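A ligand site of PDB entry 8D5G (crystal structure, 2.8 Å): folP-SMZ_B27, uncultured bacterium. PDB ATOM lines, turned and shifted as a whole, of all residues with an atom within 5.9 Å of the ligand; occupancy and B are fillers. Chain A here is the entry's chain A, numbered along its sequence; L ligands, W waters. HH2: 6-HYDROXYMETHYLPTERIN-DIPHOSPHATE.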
ATOM      1  N   ILE A  10      16.585   7.124  24.544  1.00  0.00           N
ATOM      2  CA  ILE A  10      17.022   8.442  25.002  1.00  0.00           C
ATOM      3  C   ILE A  10      17.021   8.457  26.527  1.00  0.00           C
ATOM      4  O   ILE A  10      16.077   7.999  27.167  1.00  0.00           O
ATOM      5  CB  ILE A  10      16.120   9.544  24.433  1.00  0.00           C
ATOM      6  CG1 ILE A  10      16.079   9.448  22.907  1.00  0.00           C
ATOM      7  CG2 ILE A  10      16.601  10.913  24.863  1.00  0.00           C
ATOM      8  CD1 ILE A  10      15.103  10.412  22.259  1.00  0.00           C
ATOM      9  N   ASN A  12      18.132  11.475  29.057  1.00  0.00           N
ATOM     10  CA  ASN A  12      18.661  12.809  29.325  1.00  0.00           C
ATOM     11  C   ASN A  12      18.809  13.029  30.824  1.00  0.00           C
ATOM     12  O   ASN A  12      17.872  12.761  31.585  1.00  0.00           O
ATOM     13  CB  ASN A  12      17.765  13.880  28.717  1.00  0.00           C
ATOM     14  CG  ASN A  12      17.768  13.853  27.204  1.00  0.00           C
ATOM     15  OD1 ASN A  12      18.791  14.070  26.571  1.00  0.00           O
ATOM     16  ND2 ASN A  12      16.606  13.582  26.615  1.00  0.00           N
ATOM     17  N   GLU A  46      21.408   6.029  25.040  1.00  0.00           N
ATOM     18  CA  GLU A  46      22.065   7.283  24.703  1.00  0.00           C
ATOM     19  C   GLU A  46      21.941   8.238  25.883  1.00  0.00           C
ATOM     20  O   GLU A  46      20.855   8.762  26.156  1.00  0.00           O
ATOM     21  CB  GLU A  46      21.466   7.891  23.435  1.00  0.00           C
ATOM     22  CG  GLU A  46      22.018   9.266  23.099  1.00  0.00           C
ATOM     23  CD  GLU A  46      21.396   9.859  21.845  1.00  0.00           C
ATOM     24  OE1 GLU A  46      20.311   9.376  21.445  1.00  0.00           O
ATOM     25  OE2 GLU A  46      21.991  10.783  21.264  1.00  0.00           O
ATOM     26  N   SER A  51      20.800  19.358  26.478  1.00  0.00           N
ATOM     27  CA  SER A  51      19.809  19.426  25.416  1.00  0.00           C
ATOM     28  C   SER A  51      20.279  20.412  24.341  1.00  0.00           C
ATOM     29  O   SER A  51      20.925  21.417  24.638  1.00  0.00           O
ATOM     30  CB  SER A  51      18.455  19.851  25.962  1.00  0.00           C
ATOM     31  OG  SER A  51      18.193  19.234  27.221  1.00  0.00           O
ATOM     32  N   THR A  52      19.937  20.101  23.092  1.00  0.00           N
ATOM     33  CA  THR A  52      20.394  20.905  21.970  1.00  0.00           C
ATOM     34  C   THR A  52      19.264  21.461  21.110  1.00  0.00           C
ATOM     35  O   THR A  52      19.535  22.148  20.123  1.00  0.00           O
ATOM     36  CB  THR A  52      21.345  20.085  21.081  1.00  0.00           C
ATOM     37  OG1 THR A  52      20.881  18.724  21.006  1.00  0.00           O
ATOM     38  CG2 THR A  52      22.744  20.094  21.670  1.00  0.00           C
ATOM     39  N   GLY A  53      18.002  21.191  21.459  1.00  0.00           N
ATOM     40  CA  GLY A  53      16.898  21.717  20.722  1.00  0.00           C
ATOM     41  C   GLY A  53      16.739  23.210  20.924  1.00  0.00           C
ATOM     42  O   GLY A  53      17.526  23.857  21.632  1.00  0.00           O
ATOM     43  N   ASP A  87      25.553  11.680  23.908  1.00  0.00           N
ATOM     44  CA  ASP A  87      25.175  12.822  23.091  1.00  0.00           C
ATOM     45  C   ASP A  87      25.992  14.029  23.567  1.00  0.00           C
ATOM     46  O   ASP A  87      25.656  14.658  24.580  1.00  0.00           O
ATOM     47  CB  ASP A  87      23.682  13.076  23.186  1.00  0.00           C
ATOM     48  CG  ASP A  87      23.173  13.960  22.058  1.00  0.00           C
ATOM     49  OD1 ASP A  87      23.860  14.062  21.016  1.00  0.00           O
ATOM     50  OD2 ASP A  87      22.074  14.541  22.202  1.00  0.00           O
ATOM     51  N   ASN A 106      27.229  10.786  19.672  1.00  0.00           N
ATOM     52  CA  ASN A 106      26.288  11.540  18.847  1.00  0.00           C
ATOM     53  C   ASN A 106      26.651  13.022  18.914  1.00  0.00           C
ATOM     54  O   ASN A 106      26.492  13.649  19.970  1.00  0.00           O
ATOM     55  CB  ASN A 106      24.858  11.287  19.298  1.00  0.00           C
ATOM     56  CG  ASN A 106      23.828  11.789  18.299  1.00  0.00           C
ATOM     57  OD1 ASN A 106      24.090  11.838  17.100  1.00  0.00           O
ATOM     58  ND2 ASN A 106      22.659  12.153  18.798  1.00  0.00           N
ATOM     59  N   VAL A 108      25.808  16.599  17.538  1.00  0.00           N
ATOM     60  CA  VAL A 108      24.830  17.410  16.814  1.00  0.00           C
ATOM     61  C   VAL A 108      25.494  18.432  15.907  1.00  0.00           C
ATOM     62  O   VAL A 108      24.875  18.904  14.956  1.00  0.00           O
ATOM     63  CB  VAL A 108      23.889  18.111  17.813  1.00  0.00           C
ATOM     64  CG1 VAL A 108      22.780  17.165  18.252  1.00  0.00           C
ATOM     65  CG2 VAL A 108      24.679  18.621  19.012  1.00  0.00           C
ATOM     66  N   VAL A 129      28.096   9.740  15.143  1.00  0.00           N
ATOM     67  CA  VAL A 129      26.903  10.066  14.381  1.00  0.00           C
ATOM     68  C   VAL A 129      26.969  11.547  14.026  1.00  0.00           C
ATOM     69  O   VAL A 129      26.867  12.413  14.905  1.00  0.00           O
ATOM     70  CB  VAL A 129      25.618   9.748  15.149  1.00  0.00           C
ATOM     71  CG1 VAL A 129      24.398  10.048  14.300  1.00  0.00           C
ATOM     72  CG2 VAL A 129      25.618   8.290  15.584  1.00  0.00           C
ATOM     73  N   MET A 131      25.215  14.628  12.446  1.00  0.00           N
ATOM     74  CA  MET A 131      23.863  15.079  12.141  1.00  0.00           C
ATOM     75  C   MET A 131      23.937  16.407  11.408  1.00  0.00           C
ATOM     76  O   MET A 131      24.711  17.288  11.778  1.00  0.00           O
ATOM     77  CB  MET A 131      23.022  15.245  13.415  1.00  0.00           C
ATOM     78  CG  MET A 131      21.541  15.483  13.135  1.00  0.00           C
ATOM     79  SD  MET A 131      20.649  16.277  14.487  1.00  0.00           S
ATOM     80  CE  MET A 131      21.742  17.653  14.830  1.00  0.00           C
ATOM     81  N   ASP A 178      23.273  11.323   9.938  1.00  0.00           N
ATOM     82  CA  ASP A 178      21.934  11.730  10.362  1.00  0.00           C
ATOM     83  C   ASP A 178      21.559  12.985   9.582  1.00  0.00           C
ATOM     84  O   ASP A 178      22.202  14.034   9.744  1.00  0.00           O
ATOM     85  CB  ASP A 178      21.894  11.993  11.875  1.00  0.00           C
ATOM     86  CG  ASP A 178      20.480  12.216  12.409  1.00  0.00           C
ATOM     87  OD1 ASP A 178      19.546  12.393  11.593  1.00  0.00           O
ATOM     88  OD2 ASP A 178      20.304  12.188  13.643  1.00  0.00           O
ATOM     89  N   GLY A 180      19.157  14.825  10.097  1.00  0.00           N
ATOM     90  CA  GLY A 180      18.489  15.772  10.957  1.00  0.00           C
ATOM     91  C   GLY A 180      17.004  15.832  10.665  1.00  0.00           C
ATOM     92  O   GLY A 180      16.574  15.531   9.541  1.00  0.00           O
ATOM     93  N   LEU A 181      16.197  16.190  11.668  1.00  0.00           N
ATOM     94  CA  LEU A 181      14.760  16.298  11.492  1.00  0.00           C
ATOM     95  C   LEU A 181      14.247  17.433  12.373  1.00  0.00           C
ATOM     96  O   LEU A 181      14.919  17.868  13.308  1.00  0.00           O
ATOM     97  CB  LEU A 181      14.047  14.987  11.852  1.00  0.00           C
ATOM     98  CG  LEU A 181      14.171  13.814  10.872  1.00  0.00           C
ATOM     99  CD1 LEU A 181      13.460  12.583  11.424  1.00  0.00           C
ATOM    100  CD2 LEU A 181      13.623  14.199   9.510  1.00  0.00           C
ATOM    101  N   PHE A 184      16.157  21.178  13.529  1.00  0.00           N
ATOM    102  CA  PHE A 184      17.532  21.124  13.043  1.00  0.00           C
ATOM    103  C   PHE A 184      17.606  21.358  11.543  1.00  0.00           C
ATOM    104  O   PHE A 184      18.578  21.943  11.049  1.00  0.00           O
ATOM    105  CB  PHE A 184      18.164  19.782  13.415  1.00  0.00           C
ATOM    106  CG  PHE A 184      18.352  19.587  14.882  1.00  0.00           C
ATOM    107  CD1 PHE A 184      19.367  20.242  15.557  1.00  0.00           C
ATOM    108  CD2 PHE A 184      17.516  18.746  15.605  1.00  0.00           C
ATOM    109  CE1 PHE A 184      19.543  20.071  16.919  1.00  0.00           C
ATOM    110  CE2 PHE A 184      17.680  18.568  16.962  1.00  0.00           C
ATOM    111  CZ  PHE A 184      18.706  19.232  17.619  1.00  0.00           C
ATOM    112  N   PHE A 210      21.019   7.193  10.547  1.00  0.00           N
ATOM    113  CA  PHE A 210      20.568   7.428  11.918  1.00  0.00           C
ATOM    114  C   PHE A 210      19.511   8.520  11.861  1.00  0.00           C
ATOM    115  O   PHE A 210      19.765   9.602  11.319  1.00  0.00           O
ATOM    116  CB  PHE A 210      21.768   7.855  12.785  1.00  0.00           C
ATOM    117  CG  PHE A 210      21.473   7.976  14.253  1.00  0.00           C
ATOM    118  CD1 PHE A 210      20.710   9.016  14.761  1.00  0.00           C
ATOM    119  CD2 PHE A 210      21.993   7.055  15.149  1.00  0.00           C
ATOM    120  CE1 PHE A 210      20.450   9.124  16.114  1.00  0.00           C
ATOM    121  CE2 PHE A 210      21.742   7.149  16.496  1.00  0.00           C
ATOM    122  CZ  PHE A 210      20.978   8.191  16.981  1.00  0.00           C
ATOM    123  N   LEU A 211      18.329   8.228  12.398  1.00  0.00           N
ATOM    124  CA  LEU A 211      17.237   9.191  12.388  1.00  0.00           C
ATOM    125  C   LEU A 211      16.516   9.172  13.727  1.00  0.00           C
ATOM    126  O   LEU A 211      16.487   8.150  14.415  1.00  0.00           O
ATOM    127  CB  LEU A 211      16.238   8.907  11.249  1.00  0.00           C
ATOM    128  CG  LEU A 211      16.689   9.352   9.864  1.00  0.00           C
ATOM    129  CD1 LEU A 211      17.425   8.232   9.143  1.00  0.00           C
ATOM    130  CD2 LEU A 211      15.505   9.839   9.040  1.00  0.00           C
ATOM    131  N   SER A 212      15.933  10.312  14.076  1.00  0.00           N
ATOM    132  CA  SER A 212      15.208  10.470  15.346  1.00  0.00           C
ATOM    133  C   SER A 212      14.005  11.372  15.118  1.00  0.00           C
ATOM    134  O   SER A 212      14.057  12.575  15.376  1.00  0.00           O
ATOM    135  CB  SER A 212      16.126  11.030  16.432  1.00  0.00           C
ATOM    136  OG  SER A 212      15.397  11.778  17.388  1.00  0.00           O
ATOM    137  N   PRO A 213      12.900  10.808  14.617  1.00  0.00           N
ATOM    138  CA  PRO A 213      11.644  11.576  14.572  1.00  0.00           C
ATOM    139  C   PRO A 213      11.227  12.021  15.966  1.00  0.00           C
ATOM    140  O   PRO A 213      11.153  13.223  16.246  1.00  0.00           O
ATOM    141  CB  PRO A 213      10.648  10.590  13.960  1.00  0.00           C
ATOM    142  CG  PRO A 213      11.495   9.638  13.188  1.00  0.00           C
ATOM    143  CD  PRO A 213      12.752   9.477  14.000  1.00  0.00           C
ATOM    144  N   SER A 214      10.959  11.055  16.842  1.00  0.00           N
ATOM    145  CA  SER A 214      10.834  11.235  18.292  1.00  0.00           C
ATOM    146  C   SER A 214      10.020  12.486  18.655  1.00  0.00           C
ATOM    147  O   SER A 214      10.496  13.390  19.343  1.00  0.00           O
ATOM    148  CB  SER A 214      12.211  11.290  18.944  1.00  0.00           C
ATOM    149  OG  SER A 214      12.890  12.483  18.610  1.00  0.00           O
ATOM    150  N   ARG A 215       8.776  12.508  18.185  1.00  0.00           N
ATOM    151  CA  ARG A 215       7.785  13.508  18.598  1.00  0.00           C
ATOM    152  C   ARG A 215       8.252  14.938  18.342  1.00  0.00           C
ATOM    153  O   ARG A 215       7.925  15.848  19.111  1.00  0.00           O
ATOM    154  CB  ARG A 215       7.427  13.331  20.081  1.00  0.00           C
ATOM    155  CG  ARG A 215       6.627  12.075  20.400  1.00  0.00           C
ATOM    156  CD  ARG A 215       6.208  12.070  21.855  1.00  0.00           C
ATOM    157  NE  ARG A 215       5.823  10.743  22.325  1.00  0.00           N
ATOM    158  CZ  ARG A 215       4.665  10.461  22.894  1.00  0.00           C
ATOM    159  NH1 ARG A 215       3.740  11.392  23.078  1.00  0.00           N
ATOM    160  NH2 ARG A 215       4.423   9.217  23.299  1.00  0.00           N
ATOM    161  N   LYS A 216       8.997  15.160  17.273  1.00  0.00           N
ATOM    162  CA  LYS A 216       9.520  16.498  16.993  1.00  0.00           C
ATOM    163  C   LYS A 216       8.408  17.411  16.499  1.00  0.00           C
ATOM    164  O   LYS A 216       7.219  17.049  16.482  1.00  0.00           O
ATOM    165  CB  LYS A 216      10.665  16.406  15.986  1.00  0.00           C
ATOM    166  CG  LYS A 216      12.026  16.169  16.629  1.00  0.00           C
ATOM    167  CD  LYS A 216      13.091  15.907  15.577  1.00  0.00           C
ATOM    168  CE  LYS A 216      14.480  15.940  16.181  1.00  0.00           C
ATOM    169  NZ  LYS A 216      14.844  14.629  16.785  1.00  0.00           N
ATOM    170  N   ARG A 250      16.229   6.732  17.038  1.00  0.00           N
ATOM    171  CA  ARG A 250      16.386   7.301  18.375  1.00  0.00           C
ATOM    172  C   ARG A 250      15.056   7.884  18.823  1.00  0.00           C
ATOM    173  O   ARG A 250      14.534   8.806  18.188  1.00  0.00           O
ATOM    174  CB  ARG A 250      17.495   8.361  18.365  1.00  0.00           C
ATOM    175  CG  ARG A 250      17.527   9.271  19.571  1.00  0.00           C
ATOM    176  CD  ARG A 250      18.354  10.517  19.264  1.00  0.00           C
ATOM    177  NE  ARG A 250      18.565  11.345  20.444  1.00  0.00           N
ATOM    178  CZ  ARG A 250      17.738  12.300  20.842  1.00  0.00           C
ATOM    179  NH1 ARG A 250      16.626  12.580  20.172  1.00  0.00           N
ATOM    180  NH2 ARG A 250      18.029  13.001  21.945  1.00  0.00           N
ATOM    181  N   HIS A 252      11.911   8.190  22.316  1.00  0.00           N
ATOM    182  CA  HIS A 252      11.580   8.192  23.711  1.00  0.00           C
ATOM    183  C   HIS A 252      10.609   7.075  23.958  1.00  0.00           C
ATOM    184  O   HIS A 252      10.481   6.606  25.047  1.00  0.00           O
ATOM    185  CB  HIS A 252      10.875   9.465  24.108  1.00  0.00           C
ATOM    186  CG  HIS A 252      11.758  10.673  24.155  1.00  0.00           C
ATOM    187  ND1 HIS A 252      12.639  10.911  25.181  1.00  0.00           N
ATOM    188  CD2 HIS A 252      11.868  11.722  23.314  1.00  0.00           C
ATOM    189  CE1 HIS A 252      13.265  12.049  24.970  1.00  0.00           C
ATOM    190  NE2 HIS A 252      12.822  12.559  23.841  1.00  0.00           N
HETATM  191  N1  HH2 L   1      17.366  15.448  18.171  1.00  0.00           N
HETATM  192  C2  HH2 L   1      17.512  15.967  19.387  1.00  0.00           C
HETATM  193  C3  HH2 L   1      18.701  15.762  20.107  1.00  0.00           C
HETATM  194  N4  HH2 L   1      19.675  15.055  19.569  1.00  0.00           N
HETATM  195  N5  HH2 L   1      20.515  13.806  17.768  1.00  0.00           N
HETATM  196  C6  HH2 L   1      20.369  13.279  16.519  1.00  0.00           C
HETATM  197  N6  HH2 L   1      21.520  12.535  16.071  1.00  0.00           N
HETATM  198  N7  HH2 L   1      19.210  13.473  15.803  1.00  0.00           N
HETATM  199  C8  HH2 L   1      18.228  14.184  16.336  1.00  0.00           C
HETATM  200  O8  HH2 L   1      17.239  14.342  15.727  1.00  0.00           O
HETATM  201  C9  HH2 L   1      18.374  14.719  17.617  1.00  0.00           C
HETATM  202  C10 HH2 L   1      19.532  14.527  18.312  1.00  0.00           C
HETATM  203  C11 HH2 L   1      16.283  16.757  19.865  1.00  0.00           C
HETATM  204  O4  HH2 L   1      15.141  16.127  19.417  1.00  0.00           O
HETATM  205  P1  HH2 L   1      14.063  15.596  20.495  1.00  0.00           P
HETATM  206  O1P HH2 L   1      13.271  16.789  21.067  1.00  0.00           O
HETATM  207  O2P HH2 L   1      13.106  14.622  19.834  1.00  0.00           O
HETATM  208  O3P HH2 L   1      14.854  14.808  21.726  1.00  0.00           O
HETATM  209  P2  HH2 L   1      15.070  15.500  23.266  1.00  0.00           P
HETATM  210  O4P HH2 L   1      13.708  15.606  23.972  1.00  0.00           O
HETATM  211  O5P HH2 L   1      16.009  14.589  24.068  1.00  0.00           O
HETATM  212  O6P HH2 L   1      15.691  16.888  23.123  1.00  0.00           O
HETATM  213  O   HOH W   1      17.032  12.888  13.088  1.00  0.00           O
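Ile 10 touches the ligand. Thr 52 touches the ligand (OG1 to C3, 3.8 Å). Asp 87 touches the ligand. Val 108 touches the ligand (CG1 to N4, 3.98 Å). Phe 184 touches the ligand. Phe 210 touches the ligand (CE1 to N6, 3.6 Å). Ser 212 touches the ligand (CB to O8, 3.6 Å). Hydrophobic or aromatic side chains that line the ligand: Ile 10, Val 108, Met 131, Phe 184, Phe 210 and His 252. Within 4 Å of the ligand: Ile 10, Asn 12, Thr 52, Asp 87, Asn 106, Val 108, Met 131, Asp 178, Phe 184, Phe 210, Ser 212, Ser 214, Lys 216, Arg 250 and His 252.
SD of Met 131 lies within hydrogen-bond range of N7 of the ligand (3.4 Å). A ring nitrogen (NE2) of His 252 is in hydrogen-bond range of an oxygen (O4P) of the ligand, at 3.2 Å. NZ of Lys 216 lies within salt-bridge range of O2P of the ligand, 3.5 Å away. ND2 of Asn 12 sits at hydrogen-bond distance from O5P of the ligand (2.8 Å). OD1 of Asn 106 lies within hydrogen-bond range of N6 of the ligand (2.9 Å). An oxygen (O2P) of the ligand lies within hydrogen-bond range of the side-chain hydroxyl (OG) of Ser 214 (2.5 Å). An oxygen (O5P) of the ligand lies within salt-bridge range of the guanidinium group of Arg 250 (3.3 Å). A nitrogen (N6) of the ligand is in hydrogen-bond range of the side-chain carboxylate of Asp 178. The backbone carbonyl oxygen (O) of Ser 214 sits close to an oxygen (O2P) of the ligand (2.9 Å).
OG of Ser 214 sits at hydrogen-bond distance from NZ of Lys 216. The backbone NH (N) of Arg 250 sits at hydrogen-bond distance from the backbone carbonyl oxygen (O) of Leu 211 (3.0 Å). The side-chain hydroxyl (OG) of Ser 214 lies within hydrogen-bond range of the side-chain hydroxyl (OG) of Ser 212 (2.9 Å). NH1 of Arg 250 sits at hydrogen-bond distance from OG of Ser 212, 3.1 Å away. OE2 of Glu 46 lies within hydrogen-bond range of ND2 of Asn 106 (2.9 Å). The side-chain carboxylate (OD1) of Asp 87 is in hydrogen-bond range of the side-chain amide nitrogen (ND2) of Asn 106, 3.2 Å away. The backbone carbonyl oxygen (O) of Ser 212 is in hydrogen-bond range of the side-chain amino group (NZ) of Lys 216. The backbone NH (N) of Gly 180 lies within hydrogen-bond range of the side-chain carboxylate (OD1) of Asp 178 (2.9 Å).
Water W1 lies within hydrogen-bond range of OD1 of Asp 178, N of Ser 212 and O8 of the ligand.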
